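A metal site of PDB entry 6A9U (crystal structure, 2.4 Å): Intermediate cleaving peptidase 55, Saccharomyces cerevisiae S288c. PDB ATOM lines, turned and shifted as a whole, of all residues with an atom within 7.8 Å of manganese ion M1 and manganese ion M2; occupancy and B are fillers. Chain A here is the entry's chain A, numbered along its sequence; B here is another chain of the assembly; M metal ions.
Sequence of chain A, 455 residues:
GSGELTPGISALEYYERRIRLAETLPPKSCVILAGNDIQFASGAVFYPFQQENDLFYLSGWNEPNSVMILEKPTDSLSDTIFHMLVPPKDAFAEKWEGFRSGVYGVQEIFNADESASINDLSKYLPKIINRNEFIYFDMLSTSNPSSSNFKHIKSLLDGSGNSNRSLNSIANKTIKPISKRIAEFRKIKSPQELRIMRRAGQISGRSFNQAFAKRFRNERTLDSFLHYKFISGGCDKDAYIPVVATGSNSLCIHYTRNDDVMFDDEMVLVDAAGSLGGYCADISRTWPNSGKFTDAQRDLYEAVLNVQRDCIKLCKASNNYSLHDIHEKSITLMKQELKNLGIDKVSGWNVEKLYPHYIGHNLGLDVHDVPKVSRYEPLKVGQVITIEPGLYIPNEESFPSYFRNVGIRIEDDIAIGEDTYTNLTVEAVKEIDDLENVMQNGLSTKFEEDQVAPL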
ATOM      1  N   TYR A 240     -20.108  23.135 -15.111  1.00  0.00           N
ATOM      2  CA  TYR A 240     -20.528  21.803 -15.548  1.00  0.00           C
ATOM      3  C   TYR A 240     -21.482  21.249 -14.497  1.00  0.00           C
ATOM      4  O   TYR A 240     -21.623  21.802 -13.404  1.00  0.00           O
ATOM      5  CB  TYR A 240     -19.326  20.865 -15.746  1.00  0.00           C
ATOM      6  CG  TYR A 240     -18.336  20.885 -14.601  1.00  0.00           C
ATOM      7  CD1 TYR A 240     -18.476  20.027 -13.508  1.00  0.00           C
ATOM      8  CD2 TYR A 240     -17.238  21.749 -14.614  1.00  0.00           C
ATOM      9  CE1 TYR A 240     -17.570  20.048 -12.452  1.00  0.00           C
ATOM     10  CE2 TYR A 240     -16.324  21.764 -13.558  1.00  0.00           C
ATOM     11  CZ  TYR A 240     -16.495  20.914 -12.481  1.00  0.00           C
ATOM     12  OH  TYR A 240     -15.595  20.925 -11.443  1.00  0.00           O
ATOM     13  N   VAL A 243     -20.939  16.763  -9.071  1.00  0.00           N
ATOM     14  CA  VAL A 243     -20.950  15.448  -8.420  1.00  0.00           C
ATOM     15  C   VAL A 243     -20.916  15.646  -6.909  1.00  0.00           C
ATOM     16  O   VAL A 243     -20.023  16.320  -6.388  1.00  0.00           O
ATOM     17  CB  VAL A 243     -19.766  14.583  -8.874  1.00  0.00           C
ATOM     18  CG1 VAL A 243     -19.772  13.235  -8.149  1.00  0.00           C
ATOM     19  CG2 VAL A 243     -19.774  14.369 -10.385  1.00  0.00           C
ATOM     20  N   VAL A 270     -16.662  15.489  -3.922  1.00  0.00           N
ATOM     21  CA  VAL A 270     -17.358  16.600  -4.576  1.00  0.00           C
ATOM     22  C   VAL A 270     -16.514  17.131  -5.731  1.00  0.00           C
ATOM     23  O   VAL A 270     -15.318  17.376  -5.563  1.00  0.00           O
ATOM     24  CB  VAL A 270     -17.696  17.725  -3.583  1.00  0.00           C
ATOM     25  CG1 VAL A 270     -18.260  18.936  -4.312  1.00  0.00           C
ATOM     26  CG2 VAL A 270     -18.678  17.238  -2.522  1.00  0.00           C
ATOM     27  N   ASP A 271     -17.155  17.348  -6.883  1.00  0.00           N
ATOM     28  CA  ASP A 271     -16.513  17.916  -8.082  1.00  0.00           C
ATOM     29  C   ASP A 271     -17.417  19.014  -8.647  1.00  0.00           C
ATOM     30  O   ASP A 271     -18.469  18.709  -9.210  1.00  0.00           O
ATOM     31  CB  ASP A 271     -16.277  16.817  -9.124  1.00  0.00           C
ATOM     32  CG  ASP A 271     -15.286  17.244 -10.205  1.00  0.00           C
ATOM     33  OD1 ASP A 271     -15.045  18.459 -10.364  1.00  0.00           O
ATOM     34  OD2 ASP A 271     -14.757  16.358 -10.917  1.00  0.00           O
ATOM     35  N   ALA A 272     -17.002  20.272  -8.523  1.00  0.00           N
ATOM     36  CA  ALA A 272     -17.820  21.409  -8.961  1.00  0.00           C
ATOM     37  C   ALA A 272     -16.976  22.679  -8.991  1.00  0.00           C
ATOM     38  O   ALA A 272     -15.964  22.784  -8.298  1.00  0.00           O
ATOM     39  CB  ALA A 272     -19.029  21.600  -8.032  1.00  0.00           C
ATOM     40  N   ALA A 273     -17.427  23.658  -9.791  1.00  0.00           N
ATOM     41  CA  ALA A 273     -16.747  24.934  -9.969  1.00  0.00           C
ATOM     42  C   ALA A 273     -17.624  25.874 -10.802  1.00  0.00           C
ATOM     43  O   ALA A 273     -18.623  25.449 -11.392  1.00  0.00           O
ATOM     44  CB  ALA A 273     -15.379  24.762 -10.644  1.00  0.00           C
ATOM     45  N   ALA A 281     -13.449  26.976 -14.659  1.00  0.00           N
ATOM     46  CA  ALA A 281     -12.594  26.390 -13.625  1.00  0.00           C
ATOM     47  C   ALA A 281     -13.038  24.942 -13.369  1.00  0.00           C
ATOM     48  O   ALA A 281     -14.018  24.469 -13.952  1.00  0.00           O
ATOM     49  CB  ALA A 281     -12.641  27.217 -12.341  1.00  0.00           C
ATOM     50  N   ASP A 282     -12.307  24.237 -12.489  1.00  0.00           N
ATOM     51  CA  ASP A 282     -12.529  22.805 -12.271  1.00  0.00           C
ATOM     52  C   ASP A 282     -11.790  22.272 -11.035  1.00  0.00           C
ATOM     53  O   ASP A 282     -10.550  22.271 -11.014  1.00  0.00           O
ATOM     54  CB  ASP A 282     -12.092  22.033 -13.528  1.00  0.00           C
ATOM     55  CG  ASP A 282     -12.572  20.592 -13.558  1.00  0.00           C
ATOM     56  OD1 ASP A 282     -13.219  20.134 -12.591  1.00  0.00           O
ATOM     57  OD2 ASP A 282     -12.300  19.908 -14.569  1.00  0.00           O
ATOM     58  N   ILE A 283     -12.523  21.770 -10.028  1.00  0.00           N
ATOM     59  CA  ILE A 283     -11.968  21.468  -8.708  1.00  0.00           C
ATOM     60  C   ILE A 283     -12.573  20.169  -8.156  1.00  0.00           C
ATOM     61  O   ILE A 283     -13.744  19.871  -8.376  1.00  0.00           O
ATOM     62  CB  ILE A 283     -12.216  22.642  -7.724  1.00  0.00           C
ATOM     63  CG1 ILE A 283     -11.361  23.866  -8.111  1.00  0.00           C
ATOM     64  CG2 ILE A 283     -11.928  22.250  -6.277  1.00  0.00           C
ATOM     65  CD1 ILE A 283     -11.533  25.051  -7.182  1.00  0.00           C
ATOM     66  N   SER A 284     -11.744  19.398  -7.417  1.00  0.00           N
ATOM     67  CA  SER A 284     -12.168  18.195  -6.694  1.00  0.00           C
ATOM     68  C   SER A 284     -11.550  18.141  -5.301  1.00  0.00           C
ATOM     69  O   SER A 284     -10.358  18.435  -5.145  1.00  0.00           O
ATOM     70  CB  SER A 284     -11.781  16.915  -7.459  1.00  0.00           C
ATOM     71  OG  SER A 284     -12.515  16.739  -8.659  1.00  0.00           O
ATOM     72  N   ILE A 359      -4.977  11.260 -16.561  1.00  0.00           N
ATOM     73  CA  ILE A 359      -4.410  12.151 -15.545  1.00  0.00           C
ATOM     74  C   ILE A 359      -4.936  13.593 -15.641  1.00  0.00           C
ATOM     75  O   ILE A 359      -4.958  14.300 -14.634  1.00  0.00           O
ATOM     76  CB  ILE A 359      -2.868  12.109 -15.630  1.00  0.00           C
ATOM     77  CG1 ILE A 359      -2.220  12.881 -14.463  1.00  0.00           C
ATOM     78  CG2 ILE A 359      -2.371  12.675 -16.954  1.00  0.00           C
ATOM     79  CD1 ILE A 359      -2.267  12.166 -13.134  1.00  0.00           C
ATOM     80  N   GLY A 360      -5.382  14.045 -16.817  1.00  0.00           N
ATOM     81  CA  GLY A 360      -5.843  15.421 -16.948  1.00  0.00           C
ATOM     82  C   GLY A 360      -6.187  15.798 -18.368  1.00  0.00           C
ATOM     83  O   GLY A 360      -6.337  14.928 -19.232  1.00  0.00           O
ATOM     84  N   HIS A 361      -6.315  17.107 -18.614  1.00  0.00           N
ATOM     85  CA  HIS A 361      -6.759  17.641 -19.904  1.00  0.00           C
ATOM     86  C   HIS A 361      -6.489  19.145 -19.965  1.00  0.00           C
ATOM     87  O   HIS A 361      -6.251  19.796 -18.947  1.00  0.00           O
ATOM     88  CB  HIS A 361      -8.242  17.336 -20.131  1.00  0.00           C
ATOM     89  CG  HIS A 361      -9.132  17.804 -19.008  1.00  0.00           C
ATOM     90  ND1 HIS A 361      -9.718  19.053 -18.983  1.00  0.00           N
ATOM     91  CD2 HIS A 361      -9.514  17.182 -17.871  1.00  0.00           C
ATOM     92  CE1 HIS A 361     -10.423  19.176 -17.874  1.00  0.00           C
ATOM     93  NE2 HIS A 361     -10.323  18.055 -17.186  1.00  0.00           N
ATOM     94  N   ASN A 362      -6.559  19.690 -21.189  1.00  0.00           N
ATOM     95  CA  ASN A 362      -6.484  21.133 -21.421  1.00  0.00           C
ATOM     96  C   ASN A 362      -7.767  21.823 -20.949  1.00  0.00           C
ATOM     97  O   ASN A 362      -8.849  21.227 -20.916  1.00  0.00           O
ATOM     98  CB  ASN A 362      -6.265  21.431 -22.912  1.00  0.00           C
ATOM     99  CG  ASN A 362      -4.788  21.464 -23.308  1.00  0.00           C
ATOM    100  OD1 ASN A 362      -4.097  22.464 -23.098  1.00  0.00           O
ATOM    101  ND2 ASN A 362      -4.309  20.383 -23.913  1.00  0.00           N
ATOM    102  N   LEU A 363      -7.643  23.119 -20.604  1.00  0.00           N
ATOM    103  CA  LEU A 363      -8.737  23.879 -20.010  1.00  0.00           C
ATOM    104  C   LEU A 363      -8.790  25.297 -20.573  1.00  0.00           C
ATOM    105  O   LEU A 363      -7.759  25.964 -20.685  1.00  0.00           O
ATOM    106  CB  LEU A 363      -8.590  23.956 -18.474  1.00  0.00           C
ATOM    107  CG  LEU A 363      -9.693  24.659 -17.682  1.00  0.00           C
ATOM    108  CD1 LEU A 363     -11.000  23.875 -17.698  1.00  0.00           C
ATOM    109  CD2 LEU A 363      -9.245  24.917 -16.251  1.00  0.00           C
ATOM    110  N   VAL A 367     -14.676  22.975 -21.173  1.00  0.00           N
ATOM    111  CA  VAL A 367     -14.090  22.221 -20.065  1.00  0.00           C
ATOM    112  C   VAL A 367     -13.018  21.272 -20.577  1.00  0.00           C
ATOM    113  O   VAL A 367     -11.894  21.241 -20.052  1.00  0.00           O
ATOM    114  CB  VAL A 367     -15.178  21.480 -19.270  1.00  0.00           C
ATOM    115  CG1 VAL A 367     -14.555  20.708 -18.118  1.00  0.00           C
ATOM    116  CG2 VAL A 367     -16.219  22.459 -18.748  1.00  0.00           C
ATOM    117  N   HIS A 368     -13.336  20.494 -21.607  1.00  0.00           N
ATOM    118  CA  HIS A 368     -12.341  19.692 -22.323  1.00  0.00           C
ATOM    119  C   HIS A 368     -11.916  20.500 -23.547  1.00  0.00           C
ATOM    120  O   HIS A 368     -12.397  20.312 -24.663  1.00  0.00           O
ATOM    121  CB  HIS A 368     -12.908  18.331 -22.694  1.00  0.00           C
ATOM    122  CG  HIS A 368     -13.116  17.419 -21.525  1.00  0.00           C
ATOM    123  ND1 HIS A 368     -13.897  16.290 -21.590  1.00  0.00           N
ATOM    124  CD2 HIS A 368     -12.645  17.492 -20.253  1.00  0.00           C
ATOM    125  CE1 HIS A 368     -13.898  15.690 -20.406  1.00  0.00           C
ATOM    126  NE2 HIS A 368     -13.153  16.400 -19.582  1.00  0.00           N
ATOM    127  N   THR A 386      -5.006  20.285 -16.131  1.00  0.00           N
ATOM    128  CA  THR A 386      -5.417  19.762 -14.847  1.00  0.00           C
ATOM    129  C   THR A 386      -4.587  18.533 -14.448  1.00  0.00           C
ATOM    130  O   THR A 386      -3.962  17.880 -15.290  1.00  0.00           O
ATOM    131  CB  THR A 386      -6.908  19.381 -14.843  1.00  0.00           C
ATOM    132  OG1 THR A 386      -7.137  18.310 -15.764  1.00  0.00           O
ATOM    133  CG2 THR A 386      -7.771  20.577 -15.237  1.00  0.00           C
ATOM    134  N   ILE A 387      -4.606  18.221 -13.149  1.00  0.00           N
ATOM    135  CA  ILE A 387      -3.890  17.087 -12.548  1.00  0.00           C
ATOM    136  C   ILE A 387      -4.824  16.472 -11.507  1.00  0.00           C
ATOM    137  O   ILE A 387      -5.077  17.090 -10.457  1.00  0.00           O
ATOM    138  CB  ILE A 387      -2.565  17.522 -11.898  1.00  0.00           C
ATOM    139  CG1 ILE A 387      -1.684  18.315 -12.872  1.00  0.00           C
ATOM    140  CG2 ILE A 387      -1.819  16.323 -11.321  1.00  0.00           C
ATOM    141  CD1 ILE A 387      -0.896  17.474 -13.873  1.00  0.00           C
ATOM    142  N   GLU A 388      -5.327  15.244 -11.757  1.00  0.00           N
ATOM    143  CA  GLU A 388      -6.415  14.673 -10.957  1.00  0.00           C
ATOM    144  C   GLU A 388      -6.359  13.144 -10.902  1.00  0.00           C
ATOM    145  O   GLU A 388      -7.218  12.449 -11.460  1.00  0.00           O
ATOM    146  CB  GLU A 388      -7.768  15.130 -11.507  1.00  0.00           C
ATOM    147  CG  GLU A 388      -7.926  14.998 -13.033  1.00  0.00           C
ATOM    148  CD  GLU A 388      -9.322  15.346 -13.522  1.00  0.00           C
ATOM    149  OE1 GLU A 388      -9.437  15.967 -14.605  1.00  0.00           O
ATOM    150  OE2 GLU A 388     -10.310  15.013 -12.821  1.00  0.00           O
ATOM    151  N   ARG A 409     -10.456  11.499  -4.788  1.00  0.00           N
ATOM    152  CA  ARG A 409      -9.858  12.220  -5.910  1.00  0.00           C
ATOM    153  C   ARG A 409      -9.539  13.656  -5.492  1.00  0.00           C
ATOM    154  O   ARG A 409     -10.298  14.269  -4.724  1.00  0.00           O
ATOM    155  CB  ARG A 409     -10.790  12.219  -7.132  1.00  0.00           C
ATOM    156  CG  ARG A 409     -10.194  12.868  -8.392  1.00  0.00           C
ATOM    157  CD  ARG A 409     -10.921  12.462  -9.674  1.00  0.00           C
ATOM    158  NE  ARG A 409     -12.148  13.222  -9.893  1.00  0.00           N
ATOM    159  CZ  ARG A 409     -13.362  12.684  -9.986  1.00  0.00           C
ATOM    160  NH1 ARG A 409     -13.523  11.371  -9.874  1.00  0.00           N
ATOM    161  NH2 ARG A 409     -14.415  13.458 -10.190  1.00  0.00           N
ATOM    162  N   GLU A 411      -7.870  17.438  -7.238  1.00  0.00           N
ATOM    163  CA  GLU A 411      -7.633  18.062  -8.551  1.00  0.00           C
ATOM    164  C   GLU A 411      -7.406  19.566  -8.419  1.00  0.00           C
ATOM    165  O   GLU A 411      -8.052  20.224  -7.608  1.00  0.00           O
ATOM    166  CB  GLU A 411      -8.816  17.766  -9.498  1.00  0.00           C
ATOM    167  CG  GLU A 411      -9.094  18.785 -10.626  1.00  0.00           C
ATOM    168  CD  GLU A 411     -10.200  18.330 -11.575  1.00  0.00           C
ATOM    169  OE1 GLU A 411     -10.031  18.410 -12.818  1.00  0.00           O
ATOM    170  OE2 GLU A 411     -11.244  17.856 -11.077  1.00  0.00           O
ATOM    171  N   ASP A 412      -6.471  20.100  -9.230  1.00  0.00           N
ATOM    172  CA  ASP A 412      -6.144  21.526  -9.293  1.00  0.00           C
ATOM    173  C   ASP A 412      -5.832  21.934 -10.743  1.00  0.00           C
ATOM    174  O   ASP A 412      -5.632  21.094 -11.612  1.00  0.00           O
ATOM    175  CB  ASP A 412      -4.950  21.879  -8.391  1.00  0.00           C
ATOM    176  CG  ASP A 412      -5.294  21.850  -6.903  1.00  0.00           C
ATOM    177  OD1 ASP A 412      -5.159  20.768  -6.282  1.00  0.00           O
ATOM    178  OD2 ASP A 412      -5.672  22.906  -6.343  1.00  0.00           O
ATOM    179  N   ASP A 413      -5.766  23.249 -10.988  1.00  0.00           N
ATOM    180  CA  ASP A 413      -5.500  23.806 -12.310  1.00  0.00           C
ATOM    181  C   ASP A 413      -4.153  24.524 -12.333  1.00  0.00           C
ATOM    182  O   ASP A 413      -3.895  25.399 -11.486  1.00  0.00           O
ATOM    183  CB  ASP A 413      -6.615  24.788 -12.719  1.00  0.00           C
ATOM    184  CG  ASP A 413      -8.011  24.215 -12.519  1.00  0.00           C
ATOM    185  OD1 ASP A 413      -8.186  22.979 -12.618  1.00  0.00           O
ATOM    186  OD2 ASP A 413      -8.953  25.002 -12.273  1.00  0.00           O
ATOM    187  CB  01B B   1     -14.349  17.237 -14.917  1.00  0.00           C
ATOM    188  CA  01B B   1     -13.427  16.096 -14.454  1.00  0.00           C
ATOM    189  N   01B B   1     -15.080  17.770 -13.799  1.00  0.00           N
ATOM    190  O2  01B B   1     -12.247  16.625 -13.910  1.00  0.00           O
ATOM    191  C   01B B   1     -13.059  15.175 -15.634  1.00  0.00           C
ATOM    192  C6  01B B   1     -15.350  16.747 -16.015  1.00  0.00           C
ATOM    193  C7  01B B   1     -16.468  15.795 -15.419  1.00  0.00           C
ATOM    194  C8  01B B   1     -16.305  14.419 -15.444  1.00  0.00           C
ATOM    195  C9  01B B   1     -17.295  13.580 -14.928  1.00  0.00           C
ATOM    196  C10 01B B   1     -18.456  14.122 -14.386  1.00  0.00           C
ATOM    197  C11 01B B   1     -18.634  15.512 -14.374  1.00  0.00           C
ATOM    198  C12 01B B   1     -17.640  16.338 -14.885  1.00  0.00           C
ATOM    199  O   01B B   1     -12.394  15.622 -16.601  1.00  0.00           O
ATOM    200  N   PRO B   2     -12.566  13.835 -15.615  1.00  0.00           N
ATOM    201  CA  PRO B   2     -11.624  12.927 -16.293  1.00  0.00           C
ATOM    202  C   PRO B   2     -12.036  12.634 -17.742  1.00  0.00           C
ATOM    203  O   PRO B   2     -13.187  12.294 -17.983  1.00  0.00           O
ATOM    204  CB  PRO B   2     -11.682  11.664 -15.441  1.00  0.00           C
ATOM    205  CG  PRO B   2     -12.137  12.122 -14.097  1.00  0.00           C
ATOM    206  CD  PRO B   2     -13.082  13.257 -14.361  1.00  0.00           C
ATOM    207  N   PRO B   3     -11.091  12.756 -18.673  1.00  0.00           N
ATOM    208  CA  PRO B   3     -11.414  12.527 -20.092  1.00  0.00           C
ATOM    209  C   PRO B   3     -11.805  11.086 -20.388  1.00  0.00           C
ATOM    210  O   PRO B   3     -12.926  10.817 -20.829  1.00  0.00           O
ATOM    211  CB  PRO B   3     -10.110  12.914 -20.812  1.00  0.00           C
ATOM    212  CG  PRO B   3      -9.393  13.801 -19.846  1.00  0.00           C
ATOM    213  CD  PRO B   3      -9.717  13.246 -18.492  1.00  0.00           C
HETATM  214 MN    MN M   1     -13.475  17.952 -12.350  1.00  0.00          MN
HETATM  215 MN    MN M   2     -11.166  17.946 -14.978  1.00  0.00          MN
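OG of Ser 284 sits close to OD2 of Asp 271. N of Glu 411 lies within hydrogen-bond range of O of Ser 284 (3.4 Å). The side-chain hydroxyl of Tyr 240 sits at hydrogen-bond distance from the backbone NH of Ala 272 (3.3 Å). OE2 of Glu 388 lies within salt-bridge range of NE of Arg 409, at 3.9 Å. OD1 of Asp 271 sits close to OH of Tyr 240 (2.7 Å). The backbone NH of Ile 283 lies within hydrogen-bond range of the side-chain hydroxyl of Tyr 240, at 3.5 Å. The side-chain carboxylate of Asp 413 lies within hydrogen-bond range of the backbone NH of Asp 282 (3.4 Å). ND1 of His 361 lies within hydrogen-bond range of O of Val 367 (3.3 Å).
OH of Tyr 240 touches manganese ion M1, 3.8 Å away. Five residues have an atom within 4 Å of manganese ion M1: Tyr 240, Asp 271, Asp 282, Glu 411 and 01B 1 of chain B.
Within 4 Å of manganese ion M2: Asp 282, His 361, Glu 388, Glu 411 and 01B 1 of chain B.
Manganese ion M1 is bound by N of 01B 1 of chain B (2.2 Å). Manganese ion M1 is bound by the side-chain carboxylate (OD1) of Asp 282 (2.2 Å). Manganese ion M1 is bound by O2 of 01B 1 of chain B (2.4 Å). The side-chain carboxylate (OD2) of Asp 271 binds manganese ion M1, 2.5 Å away. Manganese ion M1 is bound by OE2 of Glu 411 (2.6 Å). Manganese ion M1 is bound by the side-chain carboxylate (OD1) of Asp 271, at 2.6 Å. Manganese ion M1 has six donor atoms within binding distance.
Manganese ion M2 is bound by O2 of 01B 1 of chain B (2.0 Å), OD2 of Asp 282 (2.3 Å), NE2 of His 361 (2.4 Å), OE1 of Glu 411 (2.5 Å) and OE1 of Glu 388 (2.7 Å).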
